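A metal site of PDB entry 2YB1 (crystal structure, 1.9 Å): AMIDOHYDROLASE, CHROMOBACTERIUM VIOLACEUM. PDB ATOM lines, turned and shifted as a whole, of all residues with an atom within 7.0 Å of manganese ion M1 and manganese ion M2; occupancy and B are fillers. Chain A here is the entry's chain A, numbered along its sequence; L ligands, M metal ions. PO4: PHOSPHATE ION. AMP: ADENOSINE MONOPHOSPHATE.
Within 4 Å of manganese ion M1: His 7, His 9, Glu 64 and Asp 248.
The side-chain carboxylate (OE2) of Glu 64 binds manganese ion M2, 2.1 Å away. Manganese ion M2 is bound by an oxygen (O3) of PO4 L1. Manganese ion M2 is bound by NE2 of His 191 (2.1 Å). Manganese ion M2 is bound by ND1 of His 75 (2.2 Å). O4 of PO4 L1 is bound to manganese ion M2, 2.3 Å away.
Three residues have an atom within 4 Å of manganese ion M2: Glu 64, His 75 and His 191.
The side-chain carboxylate of Glu 64 sits close to a ring nitrogen (ND1) of His 39, 3.5 Å away. The backbone NH (N) of His 191 lies within hydrogen-bond range of the side-chain carboxylate (OE1) of Glu 218 (2.7 Å). ND1 of His 9 lies close to O of Thr 37, at 3.4 Å. The side-chain carboxylate (OD1) of Asp 14 is in hydrogen-bond range of a ring nitrogen (ND1) of His 9. The backbone carbonyl oxygen (O) of Phe 249 lies within hydrogen-bond range of the backbone NH (N) of His 9, at 3.0 Å. The side-chain carboxylate (OE2) of Glu 218 sits at hydrogen-bond distance from a ring nitrogen (ND1) of His 7. The side-chain hydroxyl (OH) of Tyr 195 lies within hydrogen-bond range of the backbone NH (N) of His 75. OD2 of Asp 248 lies within salt-bridge range of NH1 of Arg 194 (3.7 Å).
Manganese ion M1 is bound by an oxygen (O3) of PO4 L1, a ring nitrogen (NE2) of His 9, a ring nitrogen (NE2) of His 7, the side-chain carboxylate of Glu 64, the side-chain carboxylate of Asp 248 and an oxygen (O2) of PO4 L1. Manganese ion M1 has six donor atoms within binding distance.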
ATOM      1  N   HIS A   7     -21.353 -23.024   9.185  1.00  0.00           N
ATOM      2  CA  HIS A   7     -22.535 -22.367   8.624  1.00  0.00           C
ATOM      3  C   HIS A   7     -22.960 -22.931   7.256  1.00  0.00           C
ATOM      4  O   HIS A   7     -22.218 -22.800   6.297  1.00  0.00           O
ATOM      5  CB  HIS A   7     -22.211 -20.868   8.493  1.00  0.00           C
ATOM      6  CG  HIS A   7     -23.388 -19.997   8.177  1.00  0.00           C
ATOM      7  ND1 HIS A   7     -23.503 -18.710   8.656  1.00  0.00           N
ATOM      8  CD2 HIS A   7     -24.477 -20.215   7.401  1.00  0.00           C
ATOM      9  CE1 HIS A   7     -24.617 -18.175   8.208  1.00  0.00           C
ATOM     10  NE2 HIS A   7     -25.227 -19.060   7.445  1.00  0.00           N
ATOM     11  N   PHE A   8     -24.149 -23.510   7.158  1.00  0.00           N
ATOM     12  CA  PHE A   8     -24.709 -23.923   5.862  1.00  0.00           C
ATOM     13  C   PHE A   8     -26.182 -24.289   6.011  1.00  0.00           C
ATOM     14  O   PHE A   8     -26.684 -24.395   7.137  1.00  0.00           O
ATOM     15  CB  PHE A   8     -23.893 -25.086   5.220  1.00  0.00           C
ATOM     16  CG  PHE A   8     -23.671 -26.286   6.128  1.00  0.00           C
ATOM     17  CD1 PHE A   8     -24.585 -27.344   6.164  1.00  0.00           C
ATOM     18  CD2 PHE A   8     -22.499 -26.394   6.886  1.00  0.00           C
ATOM     19  CE1 PHE A   8     -24.370 -28.455   6.992  1.00  0.00           C
ATOM     20  CE2 PHE A   8     -22.278 -27.498   7.720  1.00  0.00           C
ATOM     21  CZ  PHE A   8     -23.222 -28.538   7.765  1.00  0.00           C
ATOM     22  N   HIS A   9     -26.845 -24.537   4.886  1.00  0.00           N
ATOM     23  CA  HIS A   9     -28.296 -24.676   4.837  1.00  0.00           C
ATOM     24  C   HIS A   9     -28.753 -25.956   4.161  1.00  0.00           C
ATOM     25  O   HIS A   9     -27.989 -26.585   3.425  1.00  0.00           O
ATOM     26  CB  HIS A   9     -28.924 -23.480   4.111  1.00  0.00           C
ATOM     27  CG  HIS A   9     -28.698 -22.192   4.832  1.00  0.00           C
ATOM     28  ND1 HIS A   9     -29.625 -21.670   5.713  1.00  0.00           N
ATOM     29  CD2 HIS A   9     -27.642 -21.358   4.858  1.00  0.00           C
ATOM     30  CE1 HIS A   9     -29.146 -20.556   6.226  1.00  0.00           C
ATOM     31  NE2 HIS A   9     -27.951 -20.344   5.728  1.00  0.00           N
ATOM     32  N   ASP A  14     -33.681 -22.657   3.290  1.00  0.00           N
ATOM     33  CA  ASP A  14     -33.379 -22.231   1.917  1.00  0.00           C
ATOM     34  C   ASP A  14     -32.269 -22.946   1.132  1.00  0.00           C
ATOM     35  O   ASP A  14     -31.880 -22.488   0.059  1.00  0.00           O
ATOM     36  CB  ASP A  14     -33.341 -20.699   1.762  1.00  0.00           C
ATOM     37  CG  ASP A  14     -32.133 -20.097   2.408  1.00  0.00           C
ATOM     38  OD1 ASP A  14     -31.422 -20.823   3.127  1.00  0.00           O
ATOM     39  OD2 ASP A  14     -31.903 -18.896   2.185  1.00  0.00           O
ATOM     40  N   THR A  37     -26.940 -24.830  10.018  1.00  0.00           N
ATOM     41  CA  THR A  37     -27.634 -23.692  10.600  1.00  0.00           C
ATOM     42  C   THR A  37     -28.696 -23.191   9.636  1.00  0.00           C
ATOM     43  O   THR A  37     -28.490 -22.200   8.924  1.00  0.00           O
ATOM     44  CB  THR A  37     -26.590 -22.567  10.817  1.00  0.00           C
ATOM     45  OG1 THR A  37     -25.953 -22.261   9.575  1.00  0.00           O
ATOM     46  CG2 THR A  37     -25.501 -23.039  11.757  1.00  0.00           C
ATOM     47  N   ASP A  38     -29.886 -23.759   9.750  1.00  0.00           N
ATOM     48  CA  ASP A  38     -30.998 -23.345   8.903  1.00  0.00           C
ATOM     49  C   ASP A  38     -31.629 -22.101   9.481  1.00  0.00           C
ATOM     50  O   ASP A  38     -31.547 -21.861  10.694  1.00  0.00           O
ATOM     51  CB  ASP A  38     -32.011 -24.476   8.754  1.00  0.00           C
ATOM     52  CG  ASP A  38     -31.618 -25.449   7.656  1.00  0.00           C
ATOM     53  OD1 ASP A  38     -31.426 -25.007   6.508  1.00  0.00           O
ATOM     54  OD2 ASP A  38     -31.498 -26.656   7.952  1.00  0.00           O
ATOM     55  N   HIS A  39     -32.249 -21.306   8.606  1.00  0.00           N
ATOM     56  CA  HIS A  39     -32.918 -20.073   9.033  1.00  0.00           C
ATOM     57  C   HIS A  39     -34.104 -20.354   9.938  1.00  0.00           C
ATOM     58  O   HIS A  39     -35.001 -21.108   9.559  1.00  0.00           O
ATOM     59  CB  HIS A  39     -33.452 -19.326   7.809  1.00  0.00           C
ATOM     60  CG  HIS A  39     -32.392 -18.790   6.899  1.00  0.00           C
ATOM     61  ND1 HIS A  39     -31.620 -17.698   7.232  1.00  0.00           N
ATOM     62  CD2 HIS A  39     -32.009 -19.167   5.665  1.00  0.00           C
ATOM     63  CE1 HIS A  39     -30.795 -17.429   6.229  1.00  0.00           C
ATOM     64  NE2 HIS A  39     -31.006 -18.306   5.269  1.00  0.00           N
ATOM     65  N   GLU A  64     -29.743 -20.344  12.286  1.00  0.00           N
ATOM     66  CA  GLU A  64     -29.483 -18.957  11.923  1.00  0.00           C
ATOM     67  C   GLU A  64     -30.736 -18.107  12.141  1.00  0.00           C
ATOM     68  O   GLU A  64     -31.758 -18.272  11.438  1.00  0.00           O
ATOM     69  CB  GLU A  64     -29.007 -18.842  10.461  1.00  0.00           C
ATOM     70  CG  GLU A  64     -28.663 -17.395  10.107  1.00  0.00           C
ATOM     71  CD  GLU A  64     -28.043 -17.246   8.751  1.00  0.00           C
ATOM     72  OE1 GLU A  64     -28.250 -18.126   7.903  1.00  0.00           O
ATOM     73  OE2 GLU A  64     -27.332 -16.249   8.551  1.00  0.00           O
ATOM     74  N   VAL A  74     -30.131  -8.275  10.511  1.00  0.00           N
ATOM     75  CA  VAL A  74     -28.900  -9.013  10.762  1.00  0.00           C
ATOM     76  C   VAL A  74     -29.234 -10.469  11.059  1.00  0.00           C
ATOM     77  O   VAL A  74     -30.380 -10.800  11.387  1.00  0.00           O
ATOM     78  CB  VAL A  74     -28.043  -8.406  11.914  1.00  0.00           C
ATOM     79  CG1 VAL A  74     -27.582  -6.981  11.559  1.00  0.00           C
ATOM     80  CG2 VAL A  74     -28.800  -8.419  13.213  1.00  0.00           C
ATOM     81  N   HIS A  75     -28.243 -11.347  10.904  1.00  0.00           N
ATOM     82  CA  HIS A  75     -28.441 -12.762  11.179  1.00  0.00           C
ATOM     83  C   HIS A  75     -27.527 -13.232  12.298  1.00  0.00           C
ATOM     84  O   HIS A  75     -26.316 -12.986  12.262  1.00  0.00           O
ATOM     85  CB  HIS A  75     -28.211 -13.589   9.910  1.00  0.00           C
ATOM     86  CG  HIS A  75     -29.300 -13.449   8.896  1.00  0.00           C
ATOM     87  ND1 HIS A  75     -29.186 -13.899   7.599  1.00  0.00           N
ATOM     88  CD2 HIS A  75     -30.544 -12.912   8.990  1.00  0.00           C
ATOM     89  CE1 HIS A  75     -30.300 -13.658   6.939  1.00  0.00           C
ATOM     90  NE2 HIS A  75     -31.146 -13.070   7.769  1.00  0.00           N
ATOM     91  N   ILE A  76     -28.122 -13.869  13.310  1.00  0.00           N
ATOM     92  CA  ILE A  76     -27.362 -14.368  14.454  1.00  0.00           C
ATOM     93  C   ILE A  76     -27.416 -15.890  14.465  1.00  0.00           C
ATOM     94  O   ILE A  76     -28.493 -16.484  14.623  1.00  0.00           O
ATOM     95  CB  ILE A  76     -27.930 -13.826  15.815  1.00  0.00           C
ATOM     96  CG1 ILE A  76     -27.963 -12.295  15.809  1.00  0.00           C
ATOM     97  CG2 ILE A  76     -27.143 -14.383  16.999  1.00  0.00           C
ATOM     98  CD1 ILE A  76     -26.584 -11.643  15.623  1.00  0.00           C
ATOM     99  N   VAL A  77     -26.266 -16.521  14.283  1.00  0.00           N
ATOM    100  CA  VAL A  77     -26.144 -17.972  14.345  1.00  0.00           C
ATOM    101  C   VAL A  77     -26.082 -18.455  15.800  1.00  0.00           C
ATOM    102  O   VAL A  77     -25.433 -17.810  16.638  1.00  0.00           O
ATOM    103  CB  VAL A  77     -24.870 -18.431  13.589  1.00  0.00           C
ATOM    104  CG1 VAL A  77     -24.422 -19.819  14.058  1.00  0.00           C
ATOM    105  CG2 VAL A  77     -25.109 -18.401  12.070  1.00  0.00           C
ATOM    106  N   ALA A 190     -23.426 -13.360  12.194  1.00  0.00           N
ATOM    107  CA  ALA A 190     -23.124 -14.028  10.941  1.00  0.00           C
ATOM    108  C   ALA A 190     -22.692 -13.024   9.867  1.00  0.00           C
ATOM    109  O   ALA A 190     -23.170 -11.899   9.851  1.00  0.00           O
ATOM    110  CB  ALA A 190     -24.333 -14.835  10.463  1.00  0.00           C
ATOM    111  N   HIS A 191     -21.746 -13.447   9.036  1.00  0.00           N
ATOM    112  CA  HIS A 191     -21.341 -12.707   7.837  1.00  0.00           C
ATOM    113  C   HIS A 191     -21.446 -11.181   7.967  1.00  0.00           C
ATOM    114  O   HIS A 191     -22.147 -10.527   7.211  1.00  0.00           O
ATOM    115  CB  HIS A 191     -22.090 -13.227   6.583  1.00  0.00           C
ATOM    116  CG  HIS A 191     -23.580 -13.207   6.722  1.00  0.00           C
ATOM    117  ND1 HIS A 191     -24.291 -12.051   6.928  1.00  0.00           N
ATOM    118  CD2 HIS A 191     -24.494 -14.215   6.660  1.00  0.00           C
ATOM    119  CE1 HIS A 191     -25.580 -12.338   6.999  1.00  0.00           C
ATOM    120  NE2 HIS A 191     -25.721 -13.638   6.837  1.00  0.00           N
ATOM    121  N   ARG A 194     -21.404  -8.390   5.112  1.00  0.00           N
ATOM    122  CA  ARG A 194     -22.562  -8.170   4.244  1.00  0.00           C
ATOM    123  C   ARG A 194     -23.414  -6.979   4.685  1.00  0.00           C
ATOM    124  O   ARG A 194     -24.233  -6.481   3.920  1.00  0.00           O
ATOM    125  CB  ARG A 194     -23.462  -9.413   4.167  1.00  0.00           C
ATOM    126  CG  ARG A 194     -22.835 -10.627   3.520  1.00  0.00           C
ATOM    127  CD  ARG A 194     -23.719 -11.159   2.382  1.00  0.00           C
ATOM    128  NE  ARG A 194     -25.137 -11.280   2.743  1.00  0.00           N
ATOM    129  CZ  ARG A 194     -25.787 -12.443   2.891  1.00  0.00           C
ATOM    130  NH1 ARG A 194     -25.145 -13.592   2.727  1.00  0.00           N
ATOM    131  NH2 ARG A 194     -27.080 -12.445   3.205  1.00  0.00           N
ATOM    132  N   TYR A 195     -23.239  -6.531   5.929  1.00  0.00           N
ATOM    133  CA  TYR A 195     -24.136  -5.509   6.468  1.00  0.00           C
ATOM    134  C   TYR A 195     -23.729  -4.120   5.969  1.00  0.00           C
ATOM    135  O   TYR A 195     -22.529  -3.852   5.772  1.00  0.00           O
ATOM    136  CB  TYR A 195     -24.139  -5.555   7.994  1.00  0.00           C
ATOM    137  CG  TYR A 195     -24.512  -6.916   8.572  1.00  0.00           C
ATOM    138  CD1 TYR A 195     -25.500  -7.688   7.992  1.00  0.00           C
ATOM    139  CD2 TYR A 195     -23.868  -7.411   9.701  1.00  0.00           C
ATOM    140  CE1 TYR A 195     -25.840  -8.933   8.511  1.00  0.00           C
ATOM    141  CE2 TYR A 195     -24.203  -8.645  10.239  1.00  0.00           C
ATOM    142  CZ  TYR A 195     -25.192  -9.398   9.638  1.00  0.00           C
ATOM    143  OH  TYR A 195     -25.539 -10.640  10.142  1.00  0.00           O
ATOM    144  N   GLU A 218     -18.553 -14.325  12.895  1.00  0.00           N
ATOM    145  CA  GLU A 218     -17.958 -15.018  11.759  1.00  0.00           C
ATOM    146  C   GLU A 218     -16.837 -14.177  11.190  1.00  0.00           C
ATOM    147  O   GLU A 218     -17.008 -13.014  10.848  1.00  0.00           O
ATOM    148  CB  GLU A 218     -19.015 -15.336  10.696  1.00  0.00           C
ATOM    149  CG  GLU A 218     -19.932 -16.462  11.131  1.00  0.00           C
ATOM    150  CD  GLU A 218     -20.966 -16.850  10.090  1.00  0.00           C
ATOM    151  OE1 GLU A 218     -21.140 -16.120   9.091  1.00  0.00           O
ATOM    152  OE2 GLU A 218     -21.622 -17.891  10.303  1.00  0.00           O
ATOM    153  N   SER A 223     -19.129 -15.536   2.474  1.00  0.00           N
ATOM    154  CA  SER A 223     -19.538 -14.186   2.083  1.00  0.00           C
ATOM    155  C   SER A 223     -18.456 -13.114   2.287  1.00  0.00           C
ATOM    156  O   SER A 223     -18.711 -11.932   2.066  1.00  0.00           O
ATOM    157  CB  SER A 223     -20.799 -13.751   2.854  1.00  0.00           C
ATOM    158  OG  SER A 223     -21.885 -14.654   2.642  1.00  0.00           O
ATOM    159  N   ASP A 248     -21.496 -20.896   4.419  1.00  0.00           N
ATOM    160  CA  ASP A 248     -22.820 -20.383   4.084  1.00  0.00           C
ATOM    161  C   ASP A 248     -23.331 -21.022   2.799  1.00  0.00           C
ATOM    162  O   ASP A 248     -24.065 -20.401   2.024  1.00  0.00           O
ATOM    163  CB  ASP A 248     -22.811 -18.847   3.935  1.00  0.00           C
ATOM    164  CG  ASP A 248     -24.210 -18.260   3.962  1.00  0.00           C
ATOM    165  OD1 ASP A 248     -25.152 -18.935   4.448  1.00  0.00           O
ATOM    166  OD2 ASP A 248     -24.383 -17.112   3.492  1.00  0.00           O
ATOM    167  N   PHE A 249     -22.972 -22.286   2.599  1.00  0.00           N
ATOM    168  CA  PHE A 249     -23.426 -23.052   1.443  1.00  0.00           C
ATOM    169  C   PHE A 249     -24.947 -23.185   1.386  1.00  0.00           C
ATOM    170  O   PHE A 249     -25.598 -23.468   2.391  1.00  0.00           O
ATOM    171  CB  PHE A 249     -22.770 -24.443   1.459  1.00  0.00           C
ATOM    172  CG  PHE A 249     -23.233 -25.340   0.336  1.00  0.00           C
ATOM    173  CD1 PHE A 249     -24.343 -26.162   0.499  1.00  0.00           C
ATOM    174  CD2 PHE A 249     -22.553 -25.352  -0.874  1.00  0.00           C
ATOM    175  CE1 PHE A 249     -24.778 -26.979  -0.523  1.00  0.00           C
ATOM    176  CE2 PHE A 249     -22.971 -26.168  -1.896  1.00  0.00           C
ATOM    177  CZ  PHE A 249     -24.087 -26.982  -1.736  1.00  0.00           C
ATOM    178  N   HIS A 250     -25.512 -22.969   0.188  1.00  0.00           N
ATOM    179  CA  HIS A 250     -26.944 -23.153  -0.106  1.00  0.00           C
ATOM    180  C   HIS A 250     -27.130 -24.206  -1.182  1.00  0.00           C
ATOM    181  O   HIS A 250     -27.934 -25.124  -1.036  1.00  0.00           O
ATOM    182  CB  HIS A 250     -27.629 -21.854  -0.560  1.00  0.00           C
ATOM    183  CG  HIS A 250     -27.878 -20.880   0.537  1.00  0.00           C
ATOM    184  ND1 HIS A 250     -26.860 -20.200   1.175  1.00  0.00           N
ATOM    185  CD2 HIS A 250     -29.028 -20.453   1.109  1.00  0.00           C
ATOM    186  CE1 HIS A 250     -27.369 -19.395   2.090  1.00  0.00           C
ATOM    187  NE2 HIS A 250     -28.686 -19.533   2.070  1.00  0.00           N
HETATM  188  P   PO4 L   1     -27.539 -16.255   4.457  1.00  0.00           P
HETATM  189  O1  PO4 L   1     -26.800 -15.915   3.180  1.00  0.00           O
HETATM  190  O2  PO4 L   1     -28.302 -17.528   4.254  1.00  0.00           O
HETATM  191  O3  PO4 L   1     -26.563 -16.481   5.594  1.00  0.00           O
HETATM  192  O4  PO4 L   1     -28.459 -15.112   4.802  1.00  0.00           O
HETATM  193  P   AMP L   2     -35.637 -13.878   3.709  1.00  0.00           P
HETATM  194  O1P AMP L   2     -35.548 -12.368   3.693  1.00  0.00           O
HETATM  195  O2P AMP L   2     -35.191 -14.358   5.078  1.00  0.00           O
HETATM  196  O3P AMP L   2     -36.996 -14.318   3.213  1.00  0.00           O
HETATM  197  O5' AMP L   2     -34.533 -14.258   2.626  1.00  0.00           O
HETATM  198  C5' AMP L   2     -33.167 -13.961   2.855  1.00  0.00           C
HETATM  199  C4' AMP L   2     -32.262 -14.925   2.128  1.00  0.00           C
HETATM  200  O4' AMP L   2     -32.149 -14.515   0.745  1.00  0.00           O
HETATM  201  C3' AMP L   2     -30.823 -14.968   2.626  1.00  0.00           C
HETATM  202  O3' AMP L   2     -30.656 -15.813   3.750  1.00  0.00           O
HETATM  203  C2' AMP L   2     -30.035 -15.433   1.395  1.00  0.00           C
HETATM  204  O2' AMP L   2     -30.093 -16.848   1.283  1.00  0.00           O
HETATM  205  C1' AMP L   2     -30.854 -14.821   0.253  1.00  0.00           C
HETATM  206  N9  AMP L   2     -30.235 -13.579  -0.253  1.00  0.00           N
HETATM  207  C8  AMP L   2     -30.423 -12.335   0.241  1.00  0.00           C
HETATM  208  N7  AMP L   2     -29.686 -11.428  -0.458  1.00  0.00           N
HETATM  209  C5  AMP L   2     -29.011 -12.107  -1.414  1.00  0.00           C
HETATM  210  C6  AMP L   2     -28.065 -11.775  -2.504  1.00  0.00           C
HETATM  211  N6  AMP L   2     -27.666 -10.494  -2.716  1.00  0.00           N
HETATM  212  N1  AMP L   2     -27.603 -12.781  -3.281  1.00  0.00           N
HETATM  213  C2  AMP L   2     -27.985 -14.065  -3.083  1.00  0.00           C
HETATM  214  N3  AMP L   2     -28.845 -14.443  -2.120  1.00  0.00           N
HETATM  215  C4  AMP L   2     -29.381 -13.521  -1.278  1.00  0.00           C
HETATM  216 MN    MN M   1     -26.892 -18.505   6.128  1.00  0.00          MN
HETATM  217 MN    MN M   2     -27.388 -14.987   6.859  1.00  0.00          MN
HETATM  218 MN    MN M   3     -30.128 -18.212   3.246  1.00  0.00          MN
